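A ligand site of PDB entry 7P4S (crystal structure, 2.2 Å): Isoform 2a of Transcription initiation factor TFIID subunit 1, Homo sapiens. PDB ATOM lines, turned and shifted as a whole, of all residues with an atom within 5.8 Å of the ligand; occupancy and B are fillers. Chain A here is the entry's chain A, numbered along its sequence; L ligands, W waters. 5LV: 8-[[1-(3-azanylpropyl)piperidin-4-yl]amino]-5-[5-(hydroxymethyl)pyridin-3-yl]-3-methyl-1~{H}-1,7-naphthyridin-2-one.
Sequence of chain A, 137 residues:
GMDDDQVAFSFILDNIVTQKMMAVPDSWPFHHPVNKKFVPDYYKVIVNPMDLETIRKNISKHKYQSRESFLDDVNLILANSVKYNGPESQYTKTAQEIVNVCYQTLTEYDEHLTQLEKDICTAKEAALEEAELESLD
Water W3 bridges a nitrogen (N) of the ligand and the side-chain hydroxyl (OH) of Tyr 91.
Water W1 lies within hydrogen-bond range of the side-chain hydroxyl of Tyr 42 (2.7 Å) and an oxygen (O) of the ligand (2.8 Å).
Residues that only touch the ligand: Trp 28, Pro 29, Val 34, Phe 38, Val 39, Tyr 84 and Tyr 91.
Ten residues have an atom within 4 Å of the ligand: Trp 28, Pro 29, Val 34, Asn 35, Phe 38, Val 39, Asp 41, Tyr 84, Asn 85 and Tyr 91.
Along chain A the residues within 4 Å of the ligand span positions 28 to 91.
ND2 of Asn 85 sits at hydrogen-bond distance from OG of Ser 81 (3.1 Å).
The side-chain hydroxyl of Tyr 84 sits at hydrogen-bond distance from the side-chain carboxylate of Asp 41 (2.7 Å).
OG of Ser 81 lies close to O of Tyr 91, 3.3 Å away.
The side-chain hydroxyl of Ser 89 lies close to the backbone NH of Tyr 91 (3.2 Å).
The backbone NH (N) of Asn 35 is in hydrogen-bond range of an oxygen (O1) of the ligand (2.7 Å).
ND2 of Asn 85 lies within hydrogen-bond range of O of the ligand (2.7 Å).
OD2 of Asp 41 is in salt-bridge range of N3 of the ligand, at 2.8 Å.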
ATOM      1  N   TRP A  28     -25.255  27.287 -13.618  1.00  0.00           N
ATOM      2  CA  TRP A  28     -24.050  26.565 -14.059  1.00  0.00           C
ATOM      3  C   TRP A  28     -23.966  26.381 -15.614  1.00  0.00           C
ATOM      4  O   TRP A  28     -22.858  26.561 -16.118  1.00  0.00           O
ATOM      5  CB  TRP A  28     -23.818  25.225 -13.289  1.00  0.00           C
ATOM      6  CG  TRP A  28     -24.743  24.088 -13.652  1.00  0.00           C
ATOM      7  CD1 TRP A  28     -25.856  23.683 -12.976  1.00  0.00           C
ATOM      8  CD2 TRP A  28     -24.662  23.254 -14.821  1.00  0.00           C
ATOM      9  NE1 TRP A  28     -26.487  22.671 -13.650  1.00  0.00           N
ATOM     10  CE2 TRP A  28     -25.792  22.414 -14.810  1.00  0.00           C
ATOM     11  CE3 TRP A  28     -23.761  23.162 -15.892  1.00  0.00           C
ATOM     12  CZ2 TRP A  28     -26.041  21.460 -15.820  1.00  0.00           C
ATOM     13  CZ3 TRP A  28     -24.016  22.243 -16.907  1.00  0.00           C
ATOM     14  CH2 TRP A  28     -25.130  21.389 -16.852  1.00  0.00           C
ATOM     15  N   PRO A  29     -25.046  26.164 -16.429  1.00  0.00           N
ATOM     16  CA  PRO A  29     -24.842  26.056 -17.887  1.00  0.00           C
ATOM     17  C   PRO A  29     -24.282  27.309 -18.565  1.00  0.00           C
ATOM     18  O   PRO A  29     -23.750  27.201 -19.671  1.00  0.00           O
ATOM     19  CB  PRO A  29     -26.244  25.748 -18.434  1.00  0.00           C
ATOM     20  CG  PRO A  29     -26.996  25.203 -17.292  1.00  0.00           C
ATOM     21  CD  PRO A  29     -26.478  25.942 -16.101  1.00  0.00           C
ATOM     22  N   PHE A  30     -24.408  28.494 -17.901  1.00  0.00           N
ATOM     23  CA  PHE A  30     -23.961  29.800 -18.393  1.00  0.00           C
ATOM     24  C   PHE A  30     -22.606  30.247 -17.846  1.00  0.00           C
ATOM     25  O   PHE A  30     -22.143  31.327 -18.244  1.00  0.00           O
ATOM     26  CB  PHE A  30     -25.002  30.904 -18.098  1.00  0.00           C
ATOM     27  CG  PHE A  30     -26.375  30.640 -18.656  1.00  0.00           C
ATOM     28  CD1 PHE A  30     -26.647  30.852 -20.000  1.00  0.00           C
ATOM     29  CD2 PHE A  30     -27.392  30.146 -17.841  1.00  0.00           C
ATOM     30  CE1 PHE A  30     -27.909  30.585 -20.517  1.00  0.00           C
ATOM     31  CE2 PHE A  30     -28.660  29.887 -18.363  1.00  0.00           C
ATOM     32  CZ  PHE A  30     -28.897  30.086 -19.701  1.00  0.00           C
ATOM     33  N   HIS A  32     -19.664  28.947 -18.335  1.00  0.00           N
ATOM     34  CA  HIS A  32     -18.606  28.691 -19.295  1.00  0.00           C
ATOM     35  C   HIS A  32     -19.169  28.700 -20.731  1.00  0.00           C
ATOM     36  O   HIS A  32     -20.390  28.563 -20.899  1.00  0.00           O
ATOM     37  CB  HIS A  32     -17.998  27.288 -19.016  1.00  0.00           C
ATOM     38  CG  HIS A  32     -17.518  27.099 -17.600  1.00  0.00           C
ATOM     39  ND1 HIS A  32     -16.378  27.728 -17.137  1.00  0.00           N
ATOM     40  CD2 HIS A  32     -18.056  26.385 -16.590  1.00  0.00           C
ATOM     41  CE1 HIS A  32     -16.257  27.375 -15.867  1.00  0.00           C
ATOM     42  NE2 HIS A  32     -17.236  26.535 -15.500  1.00  0.00           N
ATOM     43  N   PRO A  33     -18.307  28.740 -21.780  1.00  0.00           N
ATOM     44  CA  PRO A  33     -18.830  28.623 -23.152  1.00  0.00           C
ATOM     45  C   PRO A  33     -19.567  27.297 -23.374  1.00  0.00           C
ATOM     46  O   PRO A  33     -19.237  26.286 -22.733  1.00  0.00           O
ATOM     47  CB  PRO A  33     -17.572  28.674 -24.024  1.00  0.00           C
ATOM     48  CG  PRO A  33     -16.510  29.286 -23.168  1.00  0.00           C
ATOM     49  CD  PRO A  33     -16.826  28.852 -21.776  1.00  0.00           C
ATOM     50  N   VAL A  34     -20.585  27.309 -24.259  1.00  0.00           N
ATOM     51  CA  VAL A  34     -21.354  26.108 -24.595  1.00  0.00           C
ATOM     52  C   VAL A  34     -20.389  25.015 -25.111  1.00  0.00           C
ATOM     53  O   VAL A  34     -19.460  25.321 -25.852  1.00  0.00           O
ATOM     54  CB  VAL A  34     -22.510  26.425 -25.595  1.00  0.00           C
ATOM     55  CG1 VAL A  34     -23.139  25.159 -26.162  1.00  0.00           C
ATOM     56  CG2 VAL A  34     -23.582  27.295 -24.954  1.00  0.00           C
ATOM     57  N   ASN A  35     -20.582  23.762 -24.672  1.00  0.00           N
ATOM     58  CA  ASN A  35     -19.791  22.647 -25.138  1.00  0.00           C
ATOM     59  C   ASN A  35     -20.583  22.088 -26.317  1.00  0.00           C
ATOM     60  O   ASN A  35     -21.714  21.609 -26.134  1.00  0.00           O
ATOM     61  CB  ASN A  35     -19.569  21.605 -24.036  1.00  0.00           C
ATOM     62  CG  ASN A  35     -18.671  20.431 -24.395  1.00  0.00           C
ATOM     63  OD1 ASN A  35     -18.658  19.913 -25.521  1.00  0.00           O
ATOM     64  ND2 ASN A  35     -17.932  19.941 -23.414  1.00  0.00           N
ATOM     65  N   LYS A  36     -20.006  22.201 -27.526  1.00  0.00           N
ATOM     66  CA  LYS A  36     -20.549  21.779 -28.816  1.00  0.00           C
ATOM     67  C   LYS A  36     -21.072  20.320 -28.866  1.00  0.00           C
ATOM     68  O   LYS A  36     -21.927  20.014 -29.698  1.00  0.00           O
ATOM     69  CB  LYS A  36     -19.482  22.019 -29.904  1.00  0.00           C
ATOM     70  CG  LYS A  36     -20.029  22.276 -31.299  1.00  0.00           C
ATOM     71  CD  LYS A  36     -18.908  22.674 -32.269  1.00  0.00           C
ATOM     72  CE  LYS A  36     -18.295  21.523 -33.034  1.00  0.00           C
ATOM     73  NZ  LYS A  36     -18.984  21.286 -34.337  1.00  0.00           N
ATOM     74  N   PHE A  38     -22.912  18.586 -26.396  1.00  0.00           N
ATOM     75  CA  PHE A  38     -24.297  18.572 -25.896  1.00  0.00           C
ATOM     76  C   PHE A  38     -25.250  19.351 -26.799  1.00  0.00           C
ATOM     77  O   PHE A  38     -26.452  19.067 -26.811  1.00  0.00           O
ATOM     78  CB  PHE A  38     -24.348  19.196 -24.491  1.00  0.00           C
ATOM     79  CG  PHE A  38     -23.650  18.442 -23.390  1.00  0.00           C
ATOM     80  CD1 PHE A  38     -22.297  18.648 -23.127  1.00  0.00           C
ATOM     81  CD2 PHE A  38     -24.348  17.573 -22.565  1.00  0.00           C
ATOM     82  CE1 PHE A  38     -21.657  17.984 -22.083  1.00  0.00           C
ATOM     83  CE2 PHE A  38     -23.702  16.901 -21.515  1.00  0.00           C
ATOM     84  CZ  PHE A  38     -22.355  17.107 -21.286  1.00  0.00           C
ATOM     85  N   VAL A  39     -24.737  20.397 -27.492  1.00  0.00           N
ATOM     86  CA  VAL A  39     -25.514  21.325 -28.336  1.00  0.00           C
ATOM     87  C   VAL A  39     -24.823  21.421 -29.744  1.00  0.00           C
ATOM     88  O   VAL A  39     -24.138  22.411 -30.019  1.00  0.00           O
ATOM     89  CB  VAL A  39     -25.611  22.717 -27.620  1.00  0.00           C
ATOM     90  CG1 VAL A  39     -26.595  23.608 -28.320  1.00  0.00           C
ATOM     91  CG2 VAL A  39     -25.999  22.583 -26.160  1.00  0.00           C
ATOM     92  N   ASP A  41     -25.722  22.183 -32.870  1.00  0.00           N
ATOM     93  CA  ASP A  41     -26.078  23.305 -33.747  1.00  0.00           C
ATOM     94  C   ASP A  41     -25.932  24.707 -33.111  1.00  0.00           C
ATOM     95  O   ASP A  41     -26.321  25.694 -33.742  1.00  0.00           O
ATOM     96  CB  ASP A  41     -27.517  23.130 -34.313  1.00  0.00           C
ATOM     97  CG  ASP A  41     -28.648  23.234 -33.305  1.00  0.00           C
ATOM     98  OD1 ASP A  41     -28.445  22.863 -32.124  1.00  0.00           O
ATOM     99  OD2 ASP A  41     -29.757  23.647 -33.694  1.00  0.00           O
ATOM    100  N   TYR A  42     -25.364  24.797 -31.881  1.00  0.00           N
ATOM    101  CA  TYR A  42     -25.255  26.078 -31.173  1.00  0.00           C
ATOM    102  C   TYR A  42     -24.604  27.214 -31.964  1.00  0.00           C
ATOM    103  O   TYR A  42     -25.204  28.279 -32.078  1.00  0.00           O
ATOM    104  CB  TYR A  42     -24.537  25.941 -29.812  1.00  0.00           C
ATOM    105  CG  TYR A  42     -24.814  27.135 -28.902  1.00  0.00           C
ATOM    106  CD1 TYR A  42     -25.993  27.215 -28.173  1.00  0.00           C
ATOM    107  CD2 TYR A  42     -23.931  28.205 -28.841  1.00  0.00           C
ATOM    108  CE1 TYR A  42     -26.272  28.309 -27.355  1.00  0.00           C
ATOM    109  CE2 TYR A  42     -24.209  29.321 -28.036  1.00  0.00           C
ATOM    110  CZ  TYR A  42     -25.386  29.372 -27.306  1.00  0.00           C
ATOM    111  OH  TYR A  42     -25.690  30.444 -26.514  1.00  0.00           O
ATOM    112  N   VAL A  45     -26.611  28.687 -35.079  1.00  0.00           N
ATOM    113  CA  VAL A  45     -27.733  29.511 -34.605  1.00  0.00           C
ATOM    114  C   VAL A  45     -27.224  30.829 -34.002  1.00  0.00           C
ATOM    115  O   VAL A  45     -27.717  31.898 -34.378  1.00  0.00           O
ATOM    116  CB  VAL A  45     -28.612  28.691 -33.605  1.00  0.00           C
ATOM    117  CG1 VAL A  45     -29.701  29.560 -32.967  1.00  0.00           C
ATOM    118  CG2 VAL A  45     -29.232  27.468 -34.262  1.00  0.00           C
ATOM    119  N   SER A  81     -30.034  33.089 -25.330  1.00  0.00           N
ATOM    120  CA  SER A  81     -30.903  32.056 -24.744  1.00  0.00           C
ATOM    121  C   SER A  81     -32.309  32.173 -25.306  1.00  0.00           C
ATOM    122  O   SER A  81     -32.928  31.163 -25.538  1.00  0.00           O
ATOM    123  CB  SER A  81     -30.927  32.179 -23.216  1.00  0.00           C
ATOM    124  OG  SER A  81     -31.684  31.109 -22.660  1.00  0.00           O
ATOM    125  N   TYR A  84     -31.777  30.841 -29.184  1.00  0.00           N
ATOM    126  CA  TYR A  84     -31.525  29.422 -29.270  1.00  0.00           C
ATOM    127  C   TYR A  84     -32.581  28.559 -28.539  1.00  0.00           C
ATOM    128  O   TYR A  84     -33.025  27.569 -29.121  1.00  0.00           O
ATOM    129  CB  TYR A  84     -30.089  29.073 -28.815  1.00  0.00           C
ATOM    130  CG  TYR A  84     -29.784  27.606 -29.020  1.00  0.00           C
ATOM    131  CD1 TYR A  84     -29.695  27.062 -30.298  1.00  0.00           C
ATOM    132  CD2 TYR A  84     -29.666  26.736 -27.932  1.00  0.00           C
ATOM    133  CE1 TYR A  84     -29.501  25.703 -30.498  1.00  0.00           C
ATOM    134  CE2 TYR A  84     -29.520  25.361 -28.124  1.00  0.00           C
ATOM    135  CZ  TYR A  84     -29.425  24.846 -29.409  1.00  0.00           C
ATOM    136  OH  TYR A  84     -29.273  23.507 -29.637  1.00  0.00           O
ATOM    137  N   ASN A  85     -32.985  28.899 -27.292  1.00  0.00           N
ATOM    138  CA  ASN A  85     -33.935  28.061 -26.538  1.00  0.00           C
ATOM    139  C   ASN A  85     -35.390  28.566 -26.505  1.00  0.00           C
ATOM    140  O   ASN A  85     -36.278  27.837 -26.083  1.00  0.00           O
ATOM    141  CB  ASN A  85     -33.466  27.815 -25.107  1.00  0.00           C
ATOM    142  CG  ASN A  85     -31.994  27.566 -24.970  1.00  0.00           C
ATOM    143  OD1 ASN A  85     -31.481  26.525 -25.346  1.00  0.00           O
ATOM    144  ND2 ASN A  85     -31.303  28.516 -24.380  1.00  0.00           N
ATOM    145  N   SER A  89     -38.367  28.487 -22.368  1.00  0.00           N
ATOM    146  CA  SER A  89     -37.298  27.620 -21.880  1.00  0.00           C
ATOM    147  C   SER A  89     -36.862  27.911 -20.461  1.00  0.00           C
ATOM    148  O   SER A  89     -36.821  29.074 -20.057  1.00  0.00           O
ATOM    149  CB  SER A  89     -36.097  27.732 -22.808  1.00  0.00           C
ATOM    150  OG  SER A  89     -35.094  26.826 -22.403  1.00  0.00           O
ATOM    151  N   TYR A  91     -33.859  27.593 -19.531  1.00  0.00           N
ATOM    152  CA  TYR A  91     -32.560  28.255 -19.777  1.00  0.00           C
ATOM    153  C   TYR A  91     -32.722  29.770 -19.853  1.00  0.00           C
ATOM    154  O   TYR A  91     -31.864  30.507 -19.388  1.00  0.00           O
ATOM    155  CB  TYR A  91     -31.918  27.706 -21.061  1.00  0.00           C
ATOM    156  CG  TYR A  91     -31.369  26.306 -20.913  1.00  0.00           C
ATOM    157  CD1 TYR A  91     -30.152  26.083 -20.262  1.00  0.00           C
ATOM    158  CD2 TYR A  91     -32.059  25.208 -21.407  1.00  0.00           C
ATOM    159  CE1 TYR A  91     -29.651  24.788 -20.101  1.00  0.00           C
ATOM    160  CE2 TYR A  91     -31.573  23.919 -21.262  1.00  0.00           C
ATOM    161  CZ  TYR A  91     -30.343  23.717 -20.654  1.00  0.00           C
ATOM    162  OH  TYR A  91     -29.857  22.436 -20.480  1.00  0.00           O
HETATM  163  N1  5LV L   1     -31.052  23.430 -24.544  1.00  0.00           N
HETATM  164  N3  5LV L   1     -32.415  24.273 -33.127  1.00  0.00           N
HETATM  165  C4  5LV L   1     -27.383  22.512 -22.883  1.00  0.00           C
HETATM  166  C5  5LV L   1     -28.278  21.582 -23.394  1.00  0.00           C
HETATM  167  C6  5LV L   1     -29.780  23.180 -24.182  1.00  0.00           C
HETATM  168  C7  5LV L   1     -31.902  22.791 -25.555  1.00  0.00           C
HETATM  169  C8  5LV L   1     -31.043  22.484 -26.793  1.00  0.00           C
HETATM  170  C10 5LV L   1     -33.468  23.155 -29.595  1.00  0.00           C
HETATM  171  C13 5LV L   1     -33.760  23.396 -27.178  1.00  0.00           C
HETATM  172  C15 5LV L   1     -28.808  24.212 -23.889  1.00  0.00           C
HETATM  173  C17 5LV L   1     -26.218  22.039 -22.081  1.00  0.00           C
HETATM  174  C20 5LV L   1     -23.833  21.786 -21.767  1.00  0.00           C
HETATM  175  C21 5LV L   1     -22.423  22.099 -22.185  1.00  0.00           C
HETATM  176  C22 5LV L   1     -24.916  22.255 -22.500  1.00  0.00           C
HETATM  177  O   5LV L   1     -28.703  27.762 -23.937  1.00  0.00           O
HETATM  178  C16 5LV L   1     -28.318  26.611 -23.719  1.00  0.00           C
HETATM  179  C1  5LV L   1     -27.136  26.273 -22.950  1.00  0.00           C
HETATM  180  C   5LV L   1     -26.294  27.379 -22.386  1.00  0.00           C
HETATM  181  N4  5LV L   1     -29.058  25.553 -24.148  1.00  0.00           N
HETATM  182  C3  5LV L   1     -27.650  23.866 -23.145  1.00  0.00           C
HETATM  183  C2  5LV L   1     -26.834  24.970 -22.694  1.00  0.00           C
HETATM  184  N   5LV L   1     -29.408  21.880 -24.053  1.00  0.00           N
HETATM  185  O1  5LV L   1     -22.287  23.434 -22.593  1.00  0.00           O
HETATM  186  C19 5LV L   1     -24.121  21.062 -20.615  1.00  0.00           C
HETATM  187  N5  5LV L   1     -25.361  20.820 -20.177  1.00  0.00           N
HETATM  188  C18 5LV L   1     -26.382  21.313 -20.903  1.00  0.00           C
HETATM  189  C14 5LV L   1     -33.052  23.761 -25.879  1.00  0.00           C
HETATM  190  N2  5LV L   1     -32.810  23.284 -28.286  1.00  0.00           N
HETATM  191  C9  5LV L   1     -31.923  22.161 -27.995  1.00  0.00           C
HETATM  192  C11 5LV L   1     -32.771  23.945 -30.683  1.00  0.00           C
HETATM  193  C12 5LV L   1     -33.086  23.483 -32.085  1.00  0.00           C
HETATM  194  O   HOH W   1     -27.927  30.227 -24.977  1.00  0.00           O
HETATM  195  O   HOH W   2     -36.541  24.486 -25.801  1.00  0.00           O
HETATM  196  O   HOH W   3     -31.225  20.505 -22.462  1.00  0.00           O
HETATM  197  O   HOH W   4     -35.127  20.718 -27.885  1.00  0.00           O
HETATM  198  O   HOH W   5     -21.571  25.719 -20.821  1.00  0.00           O
